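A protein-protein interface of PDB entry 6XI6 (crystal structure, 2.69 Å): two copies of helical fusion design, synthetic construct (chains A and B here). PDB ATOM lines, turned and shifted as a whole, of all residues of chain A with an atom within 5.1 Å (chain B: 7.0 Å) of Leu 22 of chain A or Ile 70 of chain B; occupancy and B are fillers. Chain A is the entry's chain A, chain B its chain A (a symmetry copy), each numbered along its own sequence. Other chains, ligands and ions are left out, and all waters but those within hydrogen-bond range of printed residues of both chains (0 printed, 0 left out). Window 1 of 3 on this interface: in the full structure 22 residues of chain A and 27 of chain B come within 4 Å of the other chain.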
ATOM      1  N   ILE A  15      -1.905  17.012  26.160  1.00  0.00           N
ATOM      2  CA  ILE A  15      -1.812  15.754  26.895  1.00  0.00           C
ATOM      3  C   ILE A  15      -2.930  15.657  27.924  1.00  0.00           C
ATOM      4  O   ILE A  15      -3.556  14.602  28.087  1.00  0.00           O
ATOM      5  CB  ILE A  15      -0.425  15.621  27.553  1.00  0.00           C
ATOM      6  CG1 ILE A  15       0.673  15.598  26.488  1.00  0.00           C
ATOM      7  CG2 ILE A  15      -0.360  14.371  28.419  1.00  0.00           C
ATOM      8  CD1 ILE A  15       0.564  14.436  25.524  1.00  0.00           C
ATOM      9  N   ALA A  18      -6.324  15.144  26.080  1.00  0.00           N
ATOM     10  CA  ALA A  18      -6.442  13.758  25.643  1.00  0.00           C
ATOM     11  C   ALA A  18      -6.632  12.817  26.824  1.00  0.00           C
ATOM     12  O   ALA A  18      -7.278  11.772  26.686  1.00  0.00           O
ATOM     13  CB  ALA A  18      -5.212  13.354  24.831  1.00  0.00           C
ATOM     14  N   ARG A  19      -6.080  13.168  27.988  1.00  0.00           N
ATOM     15  CA  ARG A  19      -6.277  12.348  29.178  1.00  0.00           C
ATOM     16  C   ARG A  19      -7.729  12.390  29.640  1.00  0.00           C
ATOM     17  O   ARG A  19      -8.280  11.368  30.065  1.00  0.00           O
ATOM     18  CB  ARG A  19      -5.344  12.817  30.296  1.00  0.00           C
ATOM     19  CG  ARG A  19      -5.329  11.918  31.522  1.00  0.00           C
ATOM     20  CD  ARG A  19      -4.107  11.014  31.531  1.00  0.00           C
ATOM     21  NE  ARG A  19      -2.865  11.781  31.606  1.00  0.00           N
ATOM     22  CZ  ARG A  19      -1.654  11.239  31.676  1.00  0.00           C
ATOM     23  NH1 ARG A  19      -1.514   9.919  31.682  1.00  0.00           N
ATOM     24  NH2 ARG A  19      -0.581  12.015  31.740  1.00  0.00           N
ATOM     25  N   LYS A  20      -8.365  13.560  29.559  1.00  0.00           N
ATOM     26  CA  LYS A  20      -9.756  13.683  29.979  1.00  0.00           C
ATOM     27  C   LYS A  20     -10.724  13.116  28.949  1.00  0.00           C
ATOM     28  O   LYS A  20     -11.801  12.637  29.320  1.00  0.00           O
ATOM     29  CB  LYS A  20     -10.093  15.146  30.269  1.00  0.00           C
ATOM     30  CG  LYS A  20      -9.481  15.678  31.556  1.00  0.00           C
ATOM     31  CD  LYS A  20     -10.033  17.051  31.899  1.00  0.00           C
ATOM     32  CE  LYS A  20      -9.540  17.530  33.254  1.00  0.00           C
ATOM     33  NZ  LYS A  20      -8.066  17.725  33.276  1.00  0.00           N
ATOM     34  N   LEU A  21     -10.371  13.164  27.661  1.00  0.00           N
ATOM     35  CA  LEU A  21     -11.214  12.538  26.647  1.00  0.00           C
ATOM     36  C   LEU A  21     -11.293  11.032  26.858  1.00  0.00           C
ATOM     37  O   LEU A  21     -12.371  10.436  26.748  1.00  0.00           O
ATOM     38  CB  LEU A  21     -10.689  12.855  25.247  1.00  0.00           C
ATOM     39  CG  LEU A  21     -10.842  14.294  24.750  1.00  0.00           C
ATOM     40  CD1 LEU A  21     -10.357  14.416  23.313  1.00  0.00           C
ATOM     41  CD2 LEU A  21     -12.283  14.763  24.877  1.00  0.00           C
ATOM     42  N   LEU A  22     -10.157  10.400  27.163  1.00  0.00           N
ATOM     43  CA  LEU A  22     -10.165   8.975  27.471  1.00  0.00           C
ATOM     44  C   LEU A  22     -10.927   8.685  28.757  1.00  0.00           C
ATOM     45  O   LEU A  22     -11.572   7.636  28.873  1.00  0.00           O
ATOM     46  CB  LEU A  22      -8.732   8.455  27.572  1.00  0.00           C
ATOM     47  CG  LEU A  22      -8.565   6.970  27.892  1.00  0.00           C
ATOM     48  CD1 LEU A  22      -9.149   6.109  26.781  1.00  0.00           C
ATOM     49  CD2 LEU A  22      -7.101   6.646  28.119  1.00  0.00           C
ATOM     50  N   GLU A  23     -10.864   9.598  29.729  1.00  0.00           N
ATOM     51  CA  GLU A  23     -11.623   9.422  30.964  1.00  0.00           C
ATOM     52  C   GLU A  23     -13.118   9.365  30.683  1.00  0.00           C
ATOM     53  O   GLU A  23     -13.843   8.569  31.291  1.00  0.00           O
ATOM     54  CB  GLU A  23     -11.301  10.554  31.940  1.00  0.00           C
ATOM     55  CG  GLU A  23     -11.982  10.422  33.292  1.00  0.00           C
ATOM     56  CD  GLU A  23     -11.765  11.635  34.175  1.00  0.00           C
ATOM     57  OE1 GLU A  23     -11.466  12.720  33.633  1.00  0.00           O
ATOM     58  OE2 GLU A  23     -11.891  11.503  35.410  1.00  0.00           O
ATOM     59  N   ALA A  24     -13.598  10.201  29.759  1.00  0.00           N
ATOM     60  CA  ALA A  24     -15.007  10.159  29.385  1.00  0.00           C
ATOM     61  C   ALA A  24     -15.338   8.878  28.631  1.00  0.00           C
ATOM     62  O   ALA A  24     -16.385   8.266  28.868  1.00  0.00           O
ATOM     63  CB  ALA A  24     -15.364  11.386  28.547  1.00  0.00           C
ATOM     64  N   VAL A  25     -14.456   8.456  27.722  1.00  0.00           N
ATOM     65  CA  VAL A  25     -14.679   7.218  26.979  1.00  0.00           C
ATOM     66  C   VAL A  25     -14.719   6.026  27.928  1.00  0.00           C
ATOM     67  O   VAL A  25     -15.541   5.115  27.773  1.00  0.00           O
ATOM     68  CB  VAL A  25     -13.599   7.047  25.894  1.00  0.00           C
ATOM     69  CG1 VAL A  25     -13.689   5.670  25.257  1.00  0.00           C
ATOM     70  CG2 VAL A  25     -13.733   8.133  24.837  1.00  0.00           C
ATOM     71  N   ALA A  26     -13.841   6.021  28.933  1.00  0.00           N
ATOM     72  CA  ALA A  26     -13.806   4.910  29.879  1.00  0.00           C
ATOM     73  C   ALA A  26     -15.073   4.858  30.724  1.00  0.00           C
ATOM     74  O   ALA A  26     -15.583   3.771  31.020  1.00  0.00           O
ATOM     75  CB  ALA A  26     -12.569   5.018  30.771  1.00  0.00           C
ATOM     76  N   ARG A  27     -15.598   6.020  31.120  1.00  0.00           N
ATOM     77  CA  ARG A  27     -16.809   6.038  31.935  1.00  0.00           C
ATOM     78  C   ARG A  27     -18.033   5.641  31.118  1.00  0.00           C
ATOM     79  O   ARG A  27     -18.897   4.901  31.606  1.00  0.00           O
ATOM     80  CB  ARG A  27     -17.002   7.420  32.561  1.00  0.00           C
ATOM     81  CG  ARG A  27     -18.238   7.534  33.438  1.00  0.00           C
ATOM     82  CD  ARG A  27     -18.269   6.440  34.494  1.00  0.00           C
ATOM     83  NE  ARG A  27     -19.478   6.500  35.310  1.00  0.00           N
ATOM     84  CZ  ARG A  27     -19.821   5.578  36.205  1.00  0.00           C
ATOM     85  NH1 ARG A  27     -19.048   4.519  36.400  1.00  0.00           N
ATOM     86  NH2 ARG A  27     -20.940   5.715  36.903  1.00  0.00           N
ATOM     87  N   LEU B  17      -1.312  10.335  18.868  1.00  0.00           N
ATOM     88  CA  LEU B  17      -2.088  10.059  20.072  1.00  0.00           C
ATOM     89  C   LEU B  17      -3.583  10.113  19.787  1.00  0.00           C
ATOM     90  O   LEU B  17      -4.347   9.280  20.288  1.00  0.00           O
ATOM     91  CB  LEU B  17      -1.714  11.044  21.179  1.00  0.00           C
ATOM     92  CG  LEU B  17      -2.293  10.747  22.562  1.00  0.00           C
ATOM     93  CD1 LEU B  17      -1.889   9.352  23.018  1.00  0.00           C
ATOM     94  CD2 LEU B  17      -1.843  11.796  23.567  1.00  0.00           C
ATOM     95  N   LYS B  20      -4.549   6.886  18.045  1.00  0.00           N
ATOM     96  CA  LYS B  20      -4.702   5.731  18.921  1.00  0.00           C
ATOM     97  C   LYS B  20      -5.919   5.852  19.829  1.00  0.00           C
ATOM     98  O   LYS B  20      -6.507   4.830  20.202  1.00  0.00           O
ATOM     99  CB  LYS B  20      -3.438   5.533  19.758  1.00  0.00           C
ATOM    100  CG  LYS B  20      -2.254   4.991  18.972  1.00  0.00           C
ATOM    101  CD  LYS B  20      -1.112   4.607  19.896  1.00  0.00           C
ATOM    102  CE  LYS B  20       0.018   3.930  19.137  1.00  0.00           C
ATOM    103  NZ  LYS B  20       0.654   4.843  18.150  1.00  0.00           N
ATOM    104  N   LEU B  21      -6.308   7.074  20.202  1.00  0.00           N
ATOM    105  CA  LEU B  21      -7.529   7.248  20.982  1.00  0.00           C
ATOM    106  C   LEU B  21      -8.750   6.797  20.191  1.00  0.00           C
ATOM    107  O   LEU B  21      -9.640   6.131  20.732  1.00  0.00           O
ATOM    108  CB  LEU B  21      -7.682   8.706  21.416  1.00  0.00           C
ATOM    109  CG  LEU B  21      -6.711   9.227  22.477  1.00  0.00           C
ATOM    110  CD1 LEU B  21      -7.058  10.658  22.860  1.00  0.00           C
ATOM    111  CD2 LEU B  21      -6.707   8.323  23.701  1.00  0.00           C
ATOM    112  N   ALA B  24      -8.961   3.007  20.093  1.00  0.00           N
ATOM    113  CA  ALA B  24      -9.593   2.431  21.274  1.00  0.00           C
ATOM    114  C   ALA B  24     -11.105   2.612  21.233  1.00  0.00           C
ATOM    115  O   ALA B  24     -11.854   1.692  21.580  1.00  0.00           O
ATOM    116  CB  ALA B  24      -9.009   3.059  22.539  1.00  0.00           C
ATOM    117  N   VAL B  25     -11.571   3.789  20.808  1.00  0.00           N
ATOM    118  CA  VAL B  25     -13.007   4.033  20.704  1.00  0.00           C
ATOM    119  C   VAL B  25     -13.638   3.083  19.693  1.00  0.00           C
ATOM    120  O   VAL B  25     -14.737   2.558  19.912  1.00  0.00           O
ATOM    121  CB  VAL B  25     -13.272   5.507  20.342  1.00  0.00           C
ATOM    122  CG1 VAL B  25     -14.740   5.728  20.022  1.00  0.00           C
ATOM    123  CG2 VAL B  25     -12.830   6.419  21.477  1.00  0.00           C
ATOM    124  N   LEU B  28     -13.802  -0.493  21.308  1.00  0.00           N
ATOM    125  CA  LEU B  28     -14.838  -0.567  22.333  1.00  0.00           C
ATOM    126  C   LEU B  28     -16.232  -0.598  21.720  1.00  0.00           C
ATOM    127  O   LEU B  28     -17.135  -1.240  22.269  1.00  0.00           O
ATOM    128  CB  LEU B  28     -14.712   0.614  23.297  1.00  0.00           C
ATOM    129  CG  LEU B  28     -13.445   0.674  24.150  1.00  0.00           C
ATOM    130  CD1 LEU B  28     -13.394   1.973  24.940  1.00  0.00           C
ATOM    131  CD2 LEU B  28     -13.368  -0.528  25.077  1.00  0.00           C
ATOM    132  N   ILE B  62      -8.443  -2.366  27.081  1.00  0.00           N
ATOM    133  CA  ILE B  62      -8.331  -1.367  26.022  1.00  0.00           C
ATOM    134  C   ILE B  62      -8.080   0.013  26.616  1.00  0.00           C
ATOM    135  O   ILE B  62      -7.257   0.785  26.108  1.00  0.00           O
ATOM    136  CB  ILE B  62      -9.594  -1.383  25.139  1.00  0.00           C
ATOM    137  CG1 ILE B  62      -9.671  -2.682  24.333  1.00  0.00           C
ATOM    138  CG2 ILE B  62      -9.618  -0.179  24.210  1.00  0.00           C
ATOM    139  CD1 ILE B  62      -8.548  -2.849  23.336  1.00  0.00           C
ATOM    140  N   VAL B  63      -8.778   0.341  27.705  1.00  0.00           N
ATOM    141  CA  VAL B  63      -8.600   1.642  28.339  1.00  0.00           C
ATOM    142  C   VAL B  63      -7.214   1.752  28.963  1.00  0.00           C
ATOM    143  O   VAL B  63      -6.570   2.805  28.892  1.00  0.00           O
ATOM    144  CB  VAL B  63      -9.713   1.882  29.377  1.00  0.00           C
ATOM    145  CG1 VAL B  63      -9.471   3.182  30.129  1.00  0.00           C
ATOM    146  CG2 VAL B  63     -11.072   1.903  28.698  1.00  0.00           C
ATOM    147  N   GLU B  64      -6.729   0.668  29.575  1.00  0.00           N
ATOM    148  CA  GLU B  64      -5.417   0.705  30.214  1.00  0.00           C
ATOM    149  C   GLU B  64      -4.304   0.905  29.193  1.00  0.00           C
ATOM    150  O   GLU B  64      -3.362   1.668  29.438  1.00  0.00           O
ATOM    151  CB  GLU B  64      -5.188  -0.575  31.017  1.00  0.00           C
ATOM    152  CG  GLU B  64      -5.993  -0.653  32.303  1.00  0.00           C
ATOM    153  CD  GLU B  64      -5.874  -2.000  32.984  1.00  0.00           C
ATOM    154  OE1 GLU B  64      -5.210  -2.896  32.420  1.00  0.00           O
ATOM    155  OE2 GLU B  64      -6.445  -2.166  34.083  1.00  0.00           O
ATOM    156  N   GLU B  65      -4.390   0.228  28.045  1.00  0.00           N
ATOM    157  CA  GLU B  65      -3.386   0.420  27.004  1.00  0.00           C
ATOM    158  C   GLU B  65      -3.433   1.833  26.436  1.00  0.00           C
ATOM    159  O   GLU B  65      -2.400   2.363  26.013  1.00  0.00           O
ATOM    160  CB  GLU B  65      -3.576  -0.608  25.890  1.00  0.00           C
ATOM    161  CG  GLU B  65      -3.381  -2.048  26.337  1.00  0.00           C
ATOM    162  CD  GLU B  65      -1.977  -2.319  26.848  1.00  0.00           C
ATOM    163  OE1 GLU B  65      -1.020  -1.719  26.316  1.00  0.00           O
ATOM    164  OE2 GLU B  65      -1.833  -3.131  27.788  1.00  0.00           O
ATOM    165  N   ALA B  66      -4.613   2.456  26.422  1.00  0.00           N
ATOM    166  CA  ALA B  66      -4.710   3.834  25.957  1.00  0.00           C
ATOM    167  C   ALA B  66      -4.116   4.800  26.975  1.00  0.00           C
ATOM    168  O   ALA B  66      -3.513   5.811  26.599  1.00  0.00           O
ATOM    169  CB  ALA B  66      -6.167   4.185  25.656  1.00  0.00           C
ATOM    170  N   GLU B  67      -4.277   4.508  28.269  1.00  0.00           N
ATOM    171  CA  GLU B  67      -3.594   5.295  29.289  1.00  0.00           C
ATOM    172  C   GLU B  67      -2.085   5.138  29.186  1.00  0.00           C
ATOM    173  O   GLU B  67      -1.337   6.061  29.530  1.00  0.00           O
ATOM    174  CB  GLU B  67      -4.065   4.890  30.687  1.00  0.00           C
ATOM    175  CG  GLU B  67      -5.543   5.107  30.952  1.00  0.00           C
ATOM    176  CD  GLU B  67      -5.928   4.799  32.385  1.00  0.00           C
ATOM    177  OE1 GLU B  67      -5.114   5.072  33.292  1.00  0.00           O
ATOM    178  OE2 GLU B  67      -7.043   4.278  32.605  1.00  0.00           O
ATOM    179  N   GLN B  68      -1.621   3.979  28.717  1.00  0.00           N
ATOM    180  CA  GLN B  68      -0.188   3.763  28.554  1.00  0.00           C
ATOM    181  C   GLN B  68       0.360   4.574  27.386  1.00  0.00           C
ATOM    182  O   GLN B  68       1.458   5.135  27.473  1.00  0.00           O
ATOM    183  CB  GLN B  68       0.095   2.274  28.357  1.00  0.00           C
ATOM    184  CG  GLN B  68       1.538   1.867  28.601  1.00  0.00           C
ATOM    185  CD  GLN B  68       1.859   1.693  30.075  1.00  0.00           C
ATOM    186  OE1 GLN B  68       3.012   1.479  30.449  1.00  0.00           O
ATOM    187  NE2 GLN B  68       0.836   1.777  30.920  1.00  0.00           N
ATOM    188  N   GLU B  69      -0.392   4.646  26.285  1.00  0.00           N
ATOM    189  CA  GLU B  69       0.045   5.438  25.140  1.00  0.00           C
ATOM    190  C   GLU B  69       0.084   6.923  25.479  1.00  0.00           C
ATOM    191  O   GLU B  69       1.007   7.635  25.068  1.00  0.00           O
ATOM    192  CB  GLU B  69      -0.868   5.177  23.945  1.00  0.00           C
ATOM    193  CG  GLU B  69      -0.758   3.770  23.389  1.00  0.00           C
ATOM    194  CD  GLU B  69       0.611   3.484  22.803  1.00  0.00           C
ATOM    195  OE1 GLU B  69       1.220   4.414  22.231  1.00  0.00           O
ATOM    196  OE2 GLU B  69       1.083   2.334  22.920  1.00  0.00           O
ATOM    197  N   ILE B  70      -0.913   7.409  26.222  1.00  0.00           N
ATOM    198  CA  ILE B  70      -0.867   8.782  26.716  1.00  0.00           C
ATOM    199  C   ILE B  70       0.315   8.963  27.658  1.00  0.00           C
ATOM    200  O   ILE B  70       0.958  10.020  27.681  1.00  0.00           O
ATOM    201  CB  ILE B  70      -2.200   9.149  27.397  1.00  0.00           C
ATOM    202  CG1 ILE B  70      -3.356   9.047  26.400  1.00  0.00           C
ATOM    203  CG2 ILE B  70      -2.135  10.548  27.998  1.00  0.00           C
ATOM    204  CD1 ILE B  70      -4.707   9.375  26.998  1.00  0.00           C
ATOM    205  N   ARG B  71       0.627   7.927  28.442  1.00  0.00           N
ATOM    206  CA  ARG B  71       1.768   7.998  29.348  1.00  0.00           C
ATOM    207  C   ARG B  71       3.079   8.093  28.575  1.00  0.00           C
ATOM    208  O   ARG B  71       3.963   8.881  28.935  1.00  0.00           O
ATOM    209  CB  ARG B  71       1.778   6.777  30.268  1.00  0.00           C
ATOM    210  CG  ARG B  71       2.398   7.026  31.629  1.00  0.00           C
ATOM    211  CD  ARG B  71       1.324   7.266  32.675  1.00  0.00           C
ATOM    212  NE  ARG B  71       0.469   6.094  32.843  1.00  0.00           N
ATOM    213  CZ  ARG B  71      -0.591   6.049  33.641  1.00  0.00           C
ATOM    214  NH1 ARG B  71      -0.937   7.115  34.349  1.00  0.00           N
ATOM    215  NH2 ARG B  71      -1.309   4.938  33.729  1.00  0.00           N
ATOM    216  N   LYS B  72       3.223   7.297  27.513  1.00  0.00           N
ATOM    217  CA  LYS B  72       4.446   7.339  26.717  1.00  0.00           C
ATOM    218  C   LYS B  72       4.519   8.601  25.868  1.00  0.00           C
ATOM    219  O   LYS B  72       5.616   9.113  25.616  1.00  0.00           O
ATOM    220  CB  LYS B  72       4.539   6.097  25.832  1.00  0.00           C
ATOM    221  CG  LYS B  72       4.567   4.788  26.605  1.00  0.00           C
ATOM    222  CD  LYS B  72       4.549   3.592  25.668  1.00  0.00           C
ATOM    223  CE  LYS B  72       4.582   2.286  26.445  1.00  0.00           C
ATOM    224  NZ  LYS B  72       5.805   2.174  27.287  1.00  0.00           N
ATOM    225  N   ALA B  73       3.372   9.114  25.416  1.00  0.00           N
ATOM    226  CA  ALA B  73       3.376  10.351  24.643  1.00  0.00           C
ATOM    227  C   ALA B  73       3.752  11.549  25.505  1.00  0.00           C
ATOM    228  O   ALA B  73       4.351  12.507  25.004  1.00  0.00           O
ATOM    229  CB  ALA B  73       2.011  10.571  23.993  1.00  0.00           C
ATOM    230  N   GLU B  74       3.413  11.513  26.797  1.00  0.00           N
ATOM    231  CA  GLU B  74       3.767  12.617  27.682  1.00  0.00           C
ATOM    232  C   GLU B  74       5.265  12.647  27.957  1.00  0.00           C
ATOM    233  O   GLU B  74       5.880  13.720  27.962  1.00  0.00           O
ATOM    234  CB  GLU B  74       2.985  12.513  28.992  1.00  0.00           C
ATOM    235  CG  GLU B  74       3.235  13.664  29.954  1.00  0.00           C
ATOM    236  CD  GLU B  74       2.524  13.480  31.280  1.00  0.00           C
ATOM    237  OE1 GLU B  74       2.166  12.330  31.611  1.00  0.00           O
ATOM    238  OE2 GLU B  74       2.323  14.487  31.990  1.00  0.00           O
ATOM    239  N   ALA B  75       5.869  11.479  28.188  1.00  0.00           N
ATOM    240  CA  ALA B  75       7.306  11.425  28.441  1.00  0.00           C
ATOM    241  C   ALA B  75       8.098  11.854  27.213  1.00  0.00           C
ATOM    242  O   ALA B  75       9.108  12.557  27.333  1.00  0.00           O
ATOM    243  CB  ALA B  75       7.711  10.018  28.876  1.00  0.00           C
ATOM    244  N   PRO B 123       7.738   5.473  31.624  1.00  0.00           N
ATOM    245  CA  PRO B 123       6.849   6.630  31.825  1.00  0.00           C
ATOM    246  C   PRO B 123       5.763   6.402  32.863  1.00  0.00           C
ATOM    247  O   PRO B 123       5.135   7.378  33.291  1.00  0.00           O
ATOM    248  CB  PRO B 123       6.245   6.852  30.432  1.00  0.00           C
ATOM    249  CG  PRO B 123       6.314   5.512  29.781  1.00  0.00           C
ATOM    250  CD  PRO B 123       7.573   4.871  30.291  1.00  0.00           C
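The side-chain carboxylate (OE1) of Glu 74 of chain B is in salt-bridge range of the guanidinium group (NH2) of Arg 19 of chain A (2.8 Å).
The guanidinium group (NH2) of Arg 71 of chain B lies within salt-bridge range of the side-chain carboxylate (OE1) of Glu 67 of chain B.
CB of Glu 74 of chain B touches CG2 of Ile 15 of chain A (3.9 Å).
Ala 18 of chain A touches Leu 17 of chain B.
Ala 18 of chain A touches Leu 21 of chain B.
Ile 70 of chain B touches Ala 18 of chain A (CD1 to O, 3.5 Å).
O of Val 63 of chain B touches CD2 of Leu 22 of chain A (3.95 Å).
CD2 of Leu 22 of chain A touches CB of Ala 66 of chain B, 3.6 Å away.
Leu 22 of chain A touches Glu 67 of chain B (CD2 to N, 3.5 Å).
Leu 22 of chain A touches Ile 70 of chain B.
Val 25 of chain A touches Leu 28 of chain B.
Val 63 of chain B touches Ala 26 of chain A (CG1 to CB, 3.7 Å).
Of the printed residues of chain B, Leu 22 of chain A touches Val 63, Ala 66, Glu 67 and Ile 70.
Of chain A, only Ala 18, Arg 19 and Leu 22 come within 4 Å of Ile 70 of chain B.
Printed residues of chain A within 4 Å of Leu 17 of chain B: Ala 18.
Of the printed residues of chain A, Leu 21 of chain B touches Ala 18.
Printed residues of chain B within 4 Å of Val 25 of chain A: Val 25 and Leu 28.
The nearest residue of chain B that does not touch Leu 22 of chain A is Leu 21 of chain B (4.4 Å).
The nearest printed residue of chain B that does not touch Val 25 of chain A is Val 63 of chain B (5.6 Å).
Hydrophobic or aromatic side chains of chain B within 4 Å of the printed part of chain A: Leu 17, Leu 21, Val 25, Leu 28, Val 63, Ala 66 and Ile 70.
Along chain B the printed residues that touch a printed residue of chain A span positions 17 to 74.
Val 25 of chain B touches its own counterpart, Val 25 of chain A.
Of the 14 pairs that touch across the chains among the printed residues, 1 has its exchanged pair printed and touching as well.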
